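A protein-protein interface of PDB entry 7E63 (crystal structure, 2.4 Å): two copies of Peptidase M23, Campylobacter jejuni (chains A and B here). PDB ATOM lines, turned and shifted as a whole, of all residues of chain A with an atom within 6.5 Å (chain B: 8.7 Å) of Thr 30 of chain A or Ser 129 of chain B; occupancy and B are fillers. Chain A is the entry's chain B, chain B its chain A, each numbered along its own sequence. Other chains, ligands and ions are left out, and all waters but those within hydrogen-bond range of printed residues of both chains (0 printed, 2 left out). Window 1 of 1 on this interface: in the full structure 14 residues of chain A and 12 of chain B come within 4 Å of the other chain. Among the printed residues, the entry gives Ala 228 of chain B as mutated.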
ATOM      1  N   LEU A  13       7.129  17.196 -18.029  1.00  0.00           N
ATOM      2  CA  LEU A  13       8.119  16.321 -18.694  1.00  0.00           C
ATOM      3  C   LEU A  13       8.582  16.961 -19.989  1.00  0.00           C
ATOM      4  O   LEU A  13       7.841  17.793 -20.547  1.00  0.00           O
ATOM      5  CB  LEU A  13       7.517  14.951 -19.011  1.00  0.00           C
ATOM      6  CG  LEU A  13       6.987  14.091 -17.862  1.00  0.00           C
ATOM      7  CD1 LEU A  13       6.359  12.799 -18.370  1.00  0.00           C
ATOM      8  CD2 LEU A  13       8.094  13.736 -16.895  1.00  0.00           C
ATOM      9  N   PHE A  18       9.667  11.950 -26.433  1.00  0.00           N
ATOM     10  CA  PHE A  18       8.836  11.334 -25.432  1.00  0.00           C
ATOM     11  C   PHE A  18       7.919  10.327 -26.117  1.00  0.00           C
ATOM     12  O   PHE A  18       7.314  10.644 -27.134  1.00  0.00           O
ATOM     13  CB  PHE A  18       8.006  12.386 -24.719  1.00  0.00           C
ATOM     14  CG  PHE A  18       6.999  11.800 -23.792  1.00  0.00           C
ATOM     15  CD1 PHE A  18       7.367  11.397 -22.531  1.00  0.00           C
ATOM     16  CD2 PHE A  18       5.682  11.610 -24.206  1.00  0.00           C
ATOM     17  CE1 PHE A  18       6.438  10.849 -21.663  1.00  0.00           C
ATOM     18  CE2 PHE A  18       4.739  11.054 -23.350  1.00  0.00           C
ATOM     19  CZ  PHE A  18       5.124  10.672 -22.073  1.00  0.00           C
ATOM     20  N   SER A  20       6.037   7.607 -23.878  1.00  0.00           N
ATOM     21  CA  SER A  20       4.970   7.239 -22.935  1.00  0.00           C
ATOM     22  C   SER A  20       5.375   7.457 -21.480  1.00  0.00           C
ATOM     23  O   SER A  20       6.567   7.608 -21.164  1.00  0.00           O
ATOM     24  CB  SER A  20       4.481   5.791 -23.144  1.00  0.00           C
ATOM     25  OG  SER A  20       5.382   4.807 -22.648  1.00  0.00           O
ATOM     26  N   LEU A  21       4.351   7.512 -20.621  1.00  0.00           N
ATOM     27  CA  LEU A  21       4.499   7.703 -19.182  1.00  0.00           C
ATOM     28  C   LEU A  21       3.628   6.652 -18.565  1.00  0.00           C
ATOM     29  O   LEU A  21       2.460   6.588 -18.898  1.00  0.00           O
ATOM     30  CB  LEU A  21       4.006   9.088 -18.785  1.00  0.00           C
ATOM     31  CG  LEU A  21       3.906   9.409 -17.282  1.00  0.00           C
ATOM     32  CD1 LEU A  21       5.263   9.309 -16.613  1.00  0.00           C
ATOM     33  CD2 LEU A  21       3.329  10.794 -17.055  1.00  0.00           C
ATOM     34  N   ILE A  28      -0.494   6.713 -18.591  1.00  0.00           N
ATOM     35  CA  ILE A  28      -0.963   7.998 -18.068  1.00  0.00           C
ATOM     36  C   ILE A  28      -0.907   9.010 -19.183  1.00  0.00           C
ATOM     37  O   ILE A  28       0.151   9.255 -19.728  1.00  0.00           O
ATOM     38  CB  ILE A  28      -0.121   8.544 -16.900  1.00  0.00           C
ATOM     39  CG1 ILE A  28      -0.160   7.605 -15.711  1.00  0.00           C
ATOM     40  CG2 ILE A  28      -0.615   9.930 -16.481  1.00  0.00           C
ATOM     41  CD1 ILE A  28       0.799   8.053 -14.619  1.00  0.00           C
ATOM     42  N   PRO A  29      -2.049   9.615 -19.510  1.00  0.00           N
ATOM     43  CA  PRO A  29      -2.045  10.567 -20.604  1.00  0.00           C
ATOM     44  C   PRO A  29      -1.231  11.870 -20.375  1.00  0.00           C
ATOM     45  O   PRO A  29      -1.014  12.301 -19.232  1.00  0.00           O
ATOM     46  CB  PRO A  29      -3.543  10.878 -20.793  1.00  0.00           C
ATOM     47  CG  PRO A  29      -4.261   9.708 -20.222  1.00  0.00           C
ATOM     48  CD  PRO A  29      -3.412   9.243 -19.094  1.00  0.00           C
ATOM     49  N   THR A  30      -0.821  12.485 -21.482  1.00  0.00           N
ATOM     50  CA  THR A  30      -0.089  13.737 -21.465  1.00  0.00           C
ATOM     51  C   THR A  30      -0.785  14.823 -22.282  1.00  0.00           C
ATOM     52  O   THR A  30      -1.507  14.548 -23.224  1.00  0.00           O
ATOM     53  CB  THR A  30       1.359  13.536 -21.983  1.00  0.00           C
ATOM     54  OG1 THR A  30       1.337  12.894 -23.273  1.00  0.00           O
ATOM     55  CG2 THR A  30       2.174  12.667 -20.995  1.00  0.00           C
ATOM     56  N   PHE A  31      -0.573  16.069 -21.886  1.00  0.00           N
ATOM     57  CA  PHE A  31      -1.099  17.228 -22.613  1.00  0.00           C
ATOM     58  C   PHE A  31       0.020  18.305 -22.703  1.00  0.00           C
ATOM     59  O   PHE A  31       1.042  18.215 -22.025  1.00  0.00           O
ATOM     60  CB  PHE A  31      -2.459  17.717 -22.019  1.00  0.00           C
ATOM     61  CG  PHE A  31      -2.482  17.918 -20.500  1.00  0.00           C
ATOM     62  CD1 PHE A  31      -2.688  16.848 -19.631  1.00  0.00           C
ATOM     63  CD2 PHE A  31      -2.359  19.205 -19.932  1.00  0.00           C
ATOM     64  CE1 PHE A  31      -2.732  17.045 -18.258  1.00  0.00           C
ATOM     65  CE2 PHE A  31      -2.400  19.386 -18.548  1.00  0.00           C
ATOM     66  CZ  PHE A  31      -2.565  18.308 -17.717  1.00  0.00           C
ATOM     67  N   ALA A  32      -0.129  19.274 -23.590  1.00  0.00           N
ATOM     68  CA  ALA A  32       0.921  20.265 -23.791  1.00  0.00           C
ATOM     69  C   ALA A  32       0.982  21.236 -22.630  1.00  0.00           C
ATOM     70  O   ALA A  32      -0.028  21.498 -22.014  1.00  0.00           O
ATOM     71  CB  ALA A  32       0.685  21.024 -25.081  1.00  0.00           C
ATOM     72  N   ILE A  40       5.693  18.967 -21.716  1.00  0.00           N
ATOM     73  CA  ILE A  40       4.327  18.391 -21.574  1.00  0.00           C
ATOM     74  C   ILE A  40       3.948  18.147 -20.111  1.00  0.00           C
ATOM     75  O   ILE A  40       4.815  18.072 -19.236  1.00  0.00           O
ATOM     76  CB  ILE A  40       4.162  17.051 -22.322  1.00  0.00           C
ATOM     77  CG1 ILE A  40       5.323  16.107 -22.008  1.00  0.00           C
ATOM     78  CG2 ILE A  40       4.072  17.289 -23.819  1.00  0.00           C
ATOM     79  CD1 ILE A  40       5.140  14.711 -22.538  1.00  0.00           C
ATOM     80  N   LEU A  41       2.647  18.016 -19.858  1.00  0.00           N
ATOM     81  CA  LEU A  41       2.136  17.804 -18.506  1.00  0.00           C
ATOM     82  C   LEU A  41       1.365  16.492 -18.407  1.00  0.00           C
ATOM     83  O   LEU A  41       0.888  15.950 -19.402  1.00  0.00           O
ATOM     84  CB  LEU A  41       1.219  18.948 -18.079  1.00  0.00           C
ATOM     85  CG  LEU A  41       1.855  20.339 -18.031  1.00  0.00           C
ATOM     86  CD1 LEU A  41       0.774  21.416 -17.945  1.00  0.00           C
ATOM     87  CD2 LEU A  41       2.822  20.434 -16.869  1.00  0.00           C
ATOM     88  N   ALA A  42       1.263  15.987 -17.189  1.00  0.00           N
ATOM     89  CA  ALA A  42       0.458  14.835 -16.892  1.00  0.00           C
ATOM     90  C   ALA A  42      -0.035  15.001 -15.464  1.00  0.00           C
ATOM     91  O   ALA A  42       0.674  15.573 -14.599  1.00  0.00           O
ATOM     92  CB  ALA A  42       1.266  13.572 -17.022  1.00  0.00           C
ATOM     93  N   ILE A  43      -1.250  14.522 -15.212  1.00  0.00           N
ATOM     94  CA  ILE A  43      -1.807  14.639 -13.887  1.00  0.00           C
ATOM     95  C   ILE A  43      -1.711  13.278 -13.231  1.00  0.00           C
ATOM     96  O   ILE A  43      -2.086  12.281 -13.817  1.00  0.00           O
ATOM     97  CB  ILE A  43      -3.269  15.124 -13.900  1.00  0.00           C
ATOM     98  CG1 ILE A  43      -3.352  16.513 -14.516  1.00  0.00           C
ATOM     99  CG2 ILE A  43      -3.819  15.141 -12.472  1.00  0.00           C
ATOM    100  CD1 ILE A  43      -4.753  16.993 -14.814  1.00  0.00           C
ATOM    101  N   TYR A 113     -11.558   9.878 -21.693  1.00  0.00           N
ATOM    102  CA  TYR A 113     -10.530  10.888 -21.720  1.00  0.00           C
ATOM    103  C   TYR A 113     -10.697  11.616 -23.061  1.00  0.00           C
ATOM    104  O   TYR A 113     -10.584  11.008 -24.109  1.00  0.00           O
ATOM    105  CB  TYR A 113      -9.160  10.245 -21.506  1.00  0.00           C
ATOM    106  CG  TYR A 113      -8.005  11.197 -21.624  1.00  0.00           C
ATOM    107  CD1 TYR A 113      -7.422  11.431 -22.861  1.00  0.00           C
ATOM    108  CD2 TYR A 113      -7.489  11.886 -20.516  1.00  0.00           C
ATOM    109  CE1 TYR A 113      -6.355  12.307 -23.001  1.00  0.00           C
ATOM    110  CE2 TYR A 113      -6.411  12.777 -20.654  1.00  0.00           C
ATOM    111  CZ  TYR A 113      -5.864  12.995 -21.899  1.00  0.00           C
ATOM    112  OH  TYR A 113      -4.818  13.850 -22.132  1.00  0.00           O
ATOM    113  N   THR A 114     -11.083  12.893 -22.986  1.00  0.00           N
ATOM    114  CA  THR A 114     -11.180  13.788 -24.119  1.00  0.00           C
ATOM    115  C   THR A 114      -9.803  14.427 -24.304  1.00  0.00           C
ATOM    116  O   THR A 114      -9.330  15.154 -23.418  1.00  0.00           O
ATOM    117  CB  THR A 114     -12.200  14.880 -23.833  1.00  0.00           C
ATOM    118  OG1 THR A 114     -13.457  14.265 -23.583  1.00  0.00           O
ATOM    119  CG2 THR A 114     -12.361  15.810 -25.008  1.00  0.00           C
ATOM    120  N   PRO A 115      -9.135  14.153 -25.448  1.00  0.00           N
ATOM    121  CA  PRO A 115      -7.720  14.558 -25.527  1.00  0.00           C
ATOM    122  C   PRO A 115      -7.493  15.975 -26.026  1.00  0.00           C
ATOM    123  O   PRO A 115      -6.549  16.215 -26.766  1.00  0.00           O
ATOM    124  CB  PRO A 115      -7.100  13.512 -26.469  1.00  0.00           C
ATOM    125  CG  PRO A 115      -8.231  13.024 -27.299  1.00  0.00           C
ATOM    126  CD  PRO A 115      -9.511  13.220 -26.526  1.00  0.00           C
ATOM    127  N   LYS A 116      -8.356  16.902 -25.613  1.00  0.00           N
ATOM    128  CA  LYS A 116      -8.144  18.328 -25.842  1.00  0.00           C
ATOM    129  C   LYS A 116      -8.745  19.121 -24.690  1.00  0.00           C
ATOM    130  O   LYS A 116      -9.525  18.576 -23.902  1.00  0.00           O
ATOM    131  CB  LYS A 116      -8.760  18.792 -27.173  1.00  0.00           C
ATOM    132  CG  LYS A 116     -10.182  18.327 -27.440  1.00  0.00           C
ATOM    133  CD  LYS A 116     -10.690  18.782 -28.801  1.00  0.00           C
ATOM    134  CE  LYS A 116     -11.173  20.223 -28.760  1.00  0.00           C
ATOM    135  NZ  LYS A 116     -10.884  20.966 -30.033  1.00  0.00           N
ATOM    136  N   PHE A 189      -8.999  16.301 -20.869  1.00  0.00           N
ATOM    137  CA  PHE A 189      -7.873  15.673 -20.226  1.00  0.00           C
ATOM    138  C   PHE A 189      -8.262  14.910 -18.961  1.00  0.00           C
ATOM    139  O   PHE A 189      -7.538  14.939 -17.980  1.00  0.00           O
ATOM    140  CB  PHE A 189      -6.805  16.728 -19.860  1.00  0.00           C
ATOM    141  CG  PHE A 189      -6.324  17.569 -21.009  1.00  0.00           C
ATOM    142  CD1 PHE A 189      -6.081  17.022 -22.246  1.00  0.00           C
ATOM    143  CD2 PHE A 189      -6.031  18.911 -20.808  1.00  0.00           C
ATOM    144  CE1 PHE A 189      -5.602  17.804 -23.298  1.00  0.00           C
ATOM    145  CE2 PHE A 189      -5.577  19.707 -21.853  1.00  0.00           C
ATOM    146  CZ  PHE A 189      -5.356  19.153 -23.112  1.00  0.00           C
ATOM    147  N   ILE B 125      -9.248   5.835 -27.715  1.00  0.00           N
ATOM    148  CA  ILE B 125      -8.372   6.647 -28.521  1.00  0.00           C
ATOM    149  C   ILE B 125      -7.130   5.831 -28.739  1.00  0.00           C
ATOM    150  O   ILE B 125      -6.715   5.077 -27.853  1.00  0.00           O
ATOM    151  CB  ILE B 125      -8.031   8.012 -27.905  1.00  0.00           C
ATOM    152  CG1 ILE B 125      -7.540   7.875 -26.471  1.00  0.00           C
ATOM    153  CG2 ILE B 125      -9.243   8.931 -27.968  1.00  0.00           C
ATOM    154  CD1 ILE B 125      -7.104   9.198 -25.884  1.00  0.00           C
ATOM    155  N   PRO B 126      -6.524   5.969 -29.920  1.00  0.00           N
ATOM    156  CA  PRO B 126      -5.407   5.081 -30.277  1.00  0.00           C
ATOM    157  C   PRO B 126      -4.114   5.340 -29.508  1.00  0.00           C
ATOM    158  O   PRO B 126      -3.209   4.472 -29.489  1.00  0.00           O
ATOM    159  CB  PRO B 126      -5.227   5.314 -31.767  1.00  0.00           C
ATOM    160  CG  PRO B 126      -5.885   6.635 -32.061  1.00  0.00           C
ATOM    161  CD  PRO B 126      -6.955   6.830 -31.035  1.00  0.00           C
ATOM    162  N   LEU B 127      -4.018   6.498 -28.873  1.00  0.00           N
ATOM    163  CA  LEU B 127      -2.937   6.722 -27.918  1.00  0.00           C
ATOM    164  C   LEU B 127      -3.233   7.858 -26.971  1.00  0.00           C
ATOM    165  O   LEU B 127      -4.033   8.731 -27.290  1.00  0.00           O
ATOM    166  CB  LEU B 127      -1.617   7.042 -28.623  1.00  0.00           C
ATOM    167  CG  LEU B 127      -1.588   8.438 -29.239  1.00  0.00           C
ATOM    168  CD1 LEU B 127      -0.158   8.805 -29.593  1.00  0.00           C
ATOM    169  CD2 LEU B 127      -2.491   8.501 -30.469  1.00  0.00           C
ATOM    170  N   ASN B 128      -2.497   7.889 -25.857  1.00  0.00           N
ATOM    171  CA  ASN B 128      -2.832   8.736 -24.728  1.00  0.00           C
ATOM    172  C   ASN B 128      -2.201  10.118 -24.750  1.00  0.00           C
ATOM    173  O   ASN B 128      -1.645  10.556 -23.758  1.00  0.00           O
ATOM    174  CB  ASN B 128      -2.468   8.004 -23.437  1.00  0.00           C
ATOM    175  CG  ASN B 128      -3.084   6.616 -23.374  1.00  0.00           C
ATOM    176  OD1 ASN B 128      -2.398   5.635 -23.145  1.00  0.00           O
ATOM    177  ND2 ASN B 128      -4.375   6.535 -23.598  1.00  0.00           N
ATOM    178  N   SER B 129      -2.320  10.830 -25.863  1.00  0.00           N
ATOM    179  CA  SER B 129      -1.681  12.145 -25.983  1.00  0.00           C
ATOM    180  C   SER B 129      -2.744  13.220 -26.156  1.00  0.00           C
ATOM    181  O   SER B 129      -3.841  13.052 -25.653  1.00  0.00           O
ATOM    182  CB  SER B 129      -0.603  12.161 -27.102  1.00  0.00           C
ATOM    183  OG  SER B 129      -1.157  12.417 -28.366  1.00  0.00           O
ATOM    184  N   PHE B 130      -2.410  14.312 -26.833  1.00  0.00           N
ATOM    185  CA  PHE B 130      -3.283  15.457 -26.965  1.00  0.00           C
ATOM    186  C   PHE B 130      -3.433  15.839 -28.438  1.00  0.00           C
ATOM    187  O   PHE B 130      -2.619  15.445 -29.290  1.00  0.00           O
ATOM    188  CB  PHE B 130      -2.746  16.645 -26.144  1.00  0.00           C
ATOM    189  CG  PHE B 130      -1.309  17.055 -26.467  1.00  0.00           C
ATOM    190  CD1 PHE B 130      -0.242  16.318 -26.011  1.00  0.00           C
ATOM    191  CD2 PHE B 130      -1.047  18.201 -27.192  1.00  0.00           C
ATOM    192  CE1 PHE B 130       1.036  16.696 -26.271  1.00  0.00           C
ATOM    193  CE2 PHE B 130       0.249  18.575 -27.480  1.00  0.00           C
ATOM    194  CZ  PHE B 130       1.290  17.821 -27.011  1.00  0.00           C
ATOM    195  N   ILE B 131      -4.488  16.583 -28.744  1.00  0.00           N
ATOM    196  CA  ILE B 131      -4.758  16.995 -30.100  1.00  0.00           C
ATOM    197  C   ILE B 131      -3.907  18.221 -30.429  1.00  0.00           C
ATOM    198  O   ILE B 131      -3.877  19.211 -29.685  1.00  0.00           O
ATOM    199  CB  ILE B 131      -6.242  17.322 -30.284  1.00  0.00           C
ATOM    200  CG1 ILE B 131      -7.104  16.116 -29.910  1.00  0.00           C
ATOM    201  CG2 ILE B 131      -6.533  17.746 -31.717  1.00  0.00           C
ATOM    202  CD1 ILE B 131      -6.562  14.772 -30.380  1.00  0.00           C
ATOM    203  N   THR B 132      -3.196  18.147 -31.549  1.00  0.00           N
ATOM    204  CA  THR B 132      -2.454  19.305 -32.051  1.00  0.00           C
ATOM    205  C   THR B 132      -3.082  19.880 -33.312  1.00  0.00           C
ATOM    206  O   THR B 132      -2.637  20.908 -33.756  1.00  0.00           O
ATOM    207  CB  THR B 132      -1.024  18.945 -32.398  1.00  0.00           C
ATOM    208  OG1 THR B 132      -1.050  18.017 -33.482  1.00  0.00           O
ATOM    209  CG2 THR B 132      -0.358  18.288 -31.248  1.00  0.00           C
ATOM    210  N   ASP B 153      -5.319  15.001 -35.500  1.00  0.00           N
ATOM    211  CA  ASP B 153      -3.939  14.654 -35.251  1.00  0.00           C
ATOM    212  C   ASP B 153      -3.581  14.820 -33.793  1.00  0.00           C
ATOM    213  O   ASP B 153      -3.913  15.825 -33.144  1.00  0.00           O
ATOM    214  CB  ASP B 153      -2.986  15.467 -36.114  1.00  0.00           C
ATOM    215  CG  ASP B 153      -3.346  15.442 -37.588  1.00  0.00           C
ATOM    216  OD1 ASP B 153      -3.766  14.385 -38.146  1.00  0.00           O
ATOM    217  OD2 ASP B 153      -3.183  16.518 -38.195  1.00  0.00           O
ATOM    218  N   PHE B 154      -2.878  13.805 -33.313  1.00  0.00           N
ATOM    219  CA  PHE B 154      -2.363  13.731 -31.986  1.00  0.00           C
ATOM    220  C   PHE B 154      -0.852  13.925 -32.057  1.00  0.00           C
ATOM    221  O   PHE B 154      -0.184  13.401 -32.944  1.00  0.00           O
ATOM    222  CB  PHE B 154      -2.596  12.347 -31.420  1.00  0.00           C
ATOM    223  CG  PHE B 154      -4.035  12.006 -31.196  1.00  0.00           C
ATOM    224  CD1 PHE B 154      -4.881  11.752 -32.269  1.00  0.00           C
ATOM    225  CD2 PHE B 154      -4.542  11.903 -29.885  1.00  0.00           C
ATOM    226  CE1 PHE B 154      -6.204  11.416 -32.050  1.00  0.00           C
ATOM    227  CE2 PHE B 154      -5.868  11.562 -29.667  1.00  0.00           C
ATOM    228  CZ  PHE B 154      -6.700  11.318 -30.755  1.00  0.00           C
ATOM    229  N   ARG B 155      -0.340  14.665 -31.086  1.00  0.00           N
ATOM    230  CA  ARG B 155       1.061  14.742 -30.813  1.00  0.00           C
ATOM    231  C   ARG B 155       1.640  13.352 -30.692  1.00  0.00           C
ATOM    232  O   ARG B 155       1.169  12.538 -29.925  1.00  0.00           O
ATOM    233  CB  ARG B 155       1.293  15.506 -29.509  1.00  0.00           C
ATOM    234  CG  ARG B 155       2.620  15.237 -28.843  1.00  0.00           C
ATOM    235  CD  ARG B 155       3.746  15.730 -29.695  1.00  0.00           C
ATOM    236  NE  ARG B 155       5.005  15.250 -29.143  1.00  0.00           N
ATOM    237  CZ  ARG B 155       6.129  15.097 -29.844  1.00  0.00           C
ATOM    238  NH1 ARG B 155       6.174  15.371 -31.153  1.00  0.00           N
ATOM    239  NH2 ARG B 155       7.221  14.646 -29.227  1.00  0.00           N
ATOM    240  N   ALA B 156       2.689  13.103 -31.463  1.00  0.00           N
ATOM    241  CA  ALA B 156       3.448  11.878 -31.361  1.00  0.00           C
ATOM    242  C   ALA B 156       4.785  12.130 -32.017  1.00  0.00           C
ATOM    243  O   ALA B 156       4.855  12.695 -33.117  1.00  0.00           O
ATOM    244  CB  ALA B 156       2.730  10.740 -32.060  1.00  0.00           C
ATOM    245  N   ALA B 157       5.822  11.745 -31.287  1.00  0.00           N
ATOM    246  CA  ALA B 157       7.168  11.686 -31.778  1.00  0.00           C
ATOM    247  C   ALA B 157       7.252  10.411 -32.613  1.00  0.00           C
ATOM    248  O   ALA B 157       6.488   9.483 -32.405  1.00  0.00           O
ATOM    249  CB  ALA B 157       8.155  11.623 -30.612  1.00  0.00           C
ATOM    250  N   THR B 160       6.118   6.328 -31.751  1.00  0.00           N
ATOM    251  CA  THR B 160       5.118   6.148 -30.672  1.00  0.00           C
ATOM    252  C   THR B 160       4.155   4.989 -30.986  1.00  0.00           C
ATOM    253  O   THR B 160       3.552   4.977 -32.050  1.00  0.00           O
ATOM    254  CB  THR B 160       4.343   7.437 -30.404  1.00  0.00           C
ATOM    255  OG1 THR B 160       5.283   8.454 -30.116  1.00  0.00           O
ATOM    256  CG2 THR B 160       3.429   7.273 -29.214  1.00  0.00           C
ATOM    257  N   PRO B 161       4.047   4.006 -30.071  1.00  0.00           N
ATOM    258  CA  PRO B 161       3.190   2.837 -30.309  1.00  0.00           C
ATOM    259  C   PRO B 161       1.756   3.272 -30.512  1.00  0.00           C
ATOM    260  O   PRO B 161       1.280   4.121 -29.774  1.00  0.00           O
ATOM    261  CB  PRO B 161       3.308   2.025 -29.001  1.00  0.00           C
ATOM    262  CG  PRO B 161       4.589   2.467 -28.372  1.00  0.00           C
ATOM    263  CD  PRO B 161       4.741   3.915 -28.766  1.00  0.00           C
ATOM    264  N   ILE B 162       1.094   2.723 -31.519  1.00  0.00           N
ATOM    265  CA  ILE B 162      -0.295   3.077 -31.833  1.00  0.00           C
ATOM    266  C   ILE B 162      -1.191   1.850 -31.718  1.00  0.00           C
ATOM    267  O   ILE B 162      -0.913   0.806 -32.288  1.00  0.00           O
ATOM    268  CB  ILE B 162      -0.408   3.675 -33.247  1.00  0.00           C
ATOM    269  CG1 ILE B 162       0.602   4.819 -33.400  1.00  0.00           C
ATOM    270  CG2 ILE B 162      -1.843   4.139 -33.528  1.00  0.00           C
ATOM    271  CD1 ILE B 162       0.483   5.894 -32.324  1.00  0.00           C
ATOM    272  N   ALA B 228       3.452  13.010 -36.338  1.00  0.00           N
ATOM    273  CA  ALA B 228       2.141  13.129 -35.729  1.00  0.00           C
ATOM    274  C   ALA B 228       1.398  11.835 -36.032  1.00  0.00           C
ATOM    275  O   ALA B 228       1.718  11.158 -37.021  1.00  0.00           O
ATOM    276  CB  ALA B 228       1.369  14.315 -36.310  1.00  0.00           C
ATOM    277  N   LEU B 229       0.421  11.483 -35.200  1.00  0.00           N
ATOM    278  CA  LEU B 229      -0.544  10.467 -35.571  1.00  0.00           C
ATOM    279  C   LEU B 229      -1.848  11.119 -35.998  1.00  0.00           C
ATOM    280  O   LEU B 229      -2.450  11.851 -35.201  1.00  0.00           O
ATOM    281  CB  LEU B 229      -0.849   9.509 -34.442  1.00  0.00           C
ATOM    282  CG  LEU B 229      -2.010   8.599 -34.876  1.00  0.00           C
ATOM    283  CD1 LEU B 229      -1.506   7.451 -35.736  1.00  0.00           C
ATOM    284  CD2 LEU B 229      -2.781   8.079 -33.694  1.00  0.00           C
ATOM    285  N   LEU B 243     -13.587  12.118 -32.720  1.00  0.00           N
ATOM    286  CA  LEU B 243     -13.840  12.163 -31.258  1.00  0.00           C
ATOM    287  C   LEU B 243     -15.349  12.291 -30.905  1.00  0.00           C
ATOM    288  O   LEU B 243     -15.820  11.704 -29.940  1.00  0.00           O
ATOM    289  CB  LEU B 243     -13.104  13.319 -30.618  1.00  0.00           C
ATOM    290  CG  LEU B 243     -11.583  13.366 -30.754  1.00  0.00           C
ATOM    291  CD1 LEU B 243     -11.103  14.637 -30.057  1.00  0.00           C
ATOM    292  CD2 LEU B 243     -10.857  12.142 -30.200  1.00  0.00           C
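O of Asn 128 of chain B sits at hydrogen-bond distance from N of Thr 30 of chain A, at 3.1 Å.
The backbone carbonyl oxygen (O) of Pro 115 of chain A sits at hydrogen-bond distance from the backbone NH (N) of Ile 131 of chain B, at 2.9 Å.
No position is printed for both chains.
Printed residues of chain B within 4 Å of Thr 30 of chain A: Asn 128 (3.1 Å), Ser 129 (3.4 Å) and Phe 130 (3.5 Å).
Printed residues of chain B within 4 Å of Tyr 113 of chain A: Ile 125 and Ser 129.
Of the printed residues of chain B, Ala 32 of chain A touches Phe 130.
Asp 153 of chain B touches none of the printed residues of chain A.
Phe 189 of chain A touches none of the printed residues of chain B.
The nearest residue of chain B that does not touch Thr 30 of chain A is Arg 155 of chain B (6.2 Å).
Of the 19 printed residues of chain B, 7 touch a printed residue of chain A.
Printed residues of chain B that touch a printed residue of chain A: Ile 125, Asn 128, Ser 129, Phe 130, Ile 131, Phe 154 and Ala 157.
Hydrophobic or aromatic side chains of chain B within 4 Å of the printed part of chain A: Ile 125, Phe 130, Ile 131, Phe 154 and Ala 157.
Printed residues of chain A that touch a printed residue of chain B: Phe 18, Pro 29, Thr 30, Phe 31, Ala 32, Ile 40, Tyr 113 and Pro 115.
Hydrophobic or aromatic side chains of chain A that line the printed part of chain B: Pro 29, Ala 32, Ile 40, Tyr 113 and Pro 115.
Among the printed residues, no Asp or Glu carboxylate lies within 4 Å of a Lys or Arg side-chain nitrogen of the other chain.
The backbone carbonyl oxygen of Phe 31 of chain A sits at hydrogen-bond distance from the backbone NH of Leu 41 of chain A (2.7 Å).
The side-chain hydroxyl (OG1) of Thr 160 of chain B sits at hydrogen-bond distance from the backbone carbonyl oxygen (O) of Ala 157 of chain B (2.8 Å).
The side-chain hydroxyl (OG) of Ser 129 of chain B is in hydrogen-bond range of the backbone carbonyl oxygen (O) of Arg 155 of chain B (2.8 Å).
The backbone NH of Phe 154 of chain B is in hydrogen-bond range of the backbone carbonyl oxygen of Leu 229 of chain B (2.8 Å).
The backbone NH (N) of Arg 155 of chain B sits at hydrogen-bond distance from the backbone carbonyl oxygen (O) of Phe 130 of chain B (3.0 Å).
N of Ile 40 of chain A is in hydrogen-bond range of O of Leu 13 of chain A (2.7 Å).
Among the printed residues, merely in contact across the chains: Phe 18 of chain A with Ala 157 of chain B (3.7 Å), Pro 29 of chain A with Asn 128 of chain B (3.2 Å), Thr 30 of chain A with Ser 129 of chain B (3.4 Å), Thr 30 of chain A with Phe 130 of chain B (3.5 Å), Phe 31 of chain A with Phe 130 of chain B (3.6 Å), Ala 32 of chain A with Phe 130 of chain B (3.5 Å), Ile 40 of chain A with Phe 130 of chain B (3.9 Å), Tyr 113 of chain A with Ile 125 of chain B (3.8 Å), Tyr 113 of chain A with Ser 129 of chain B (3.7 Å), Pro 115 of chain A with Ser 129 of chain B (3.4 Å), Pro 115 of chain A with Phe 130 of chain B (3.4 Å) and Pro 115 of chain A with Phe 154 of chain B (3.7 Å).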
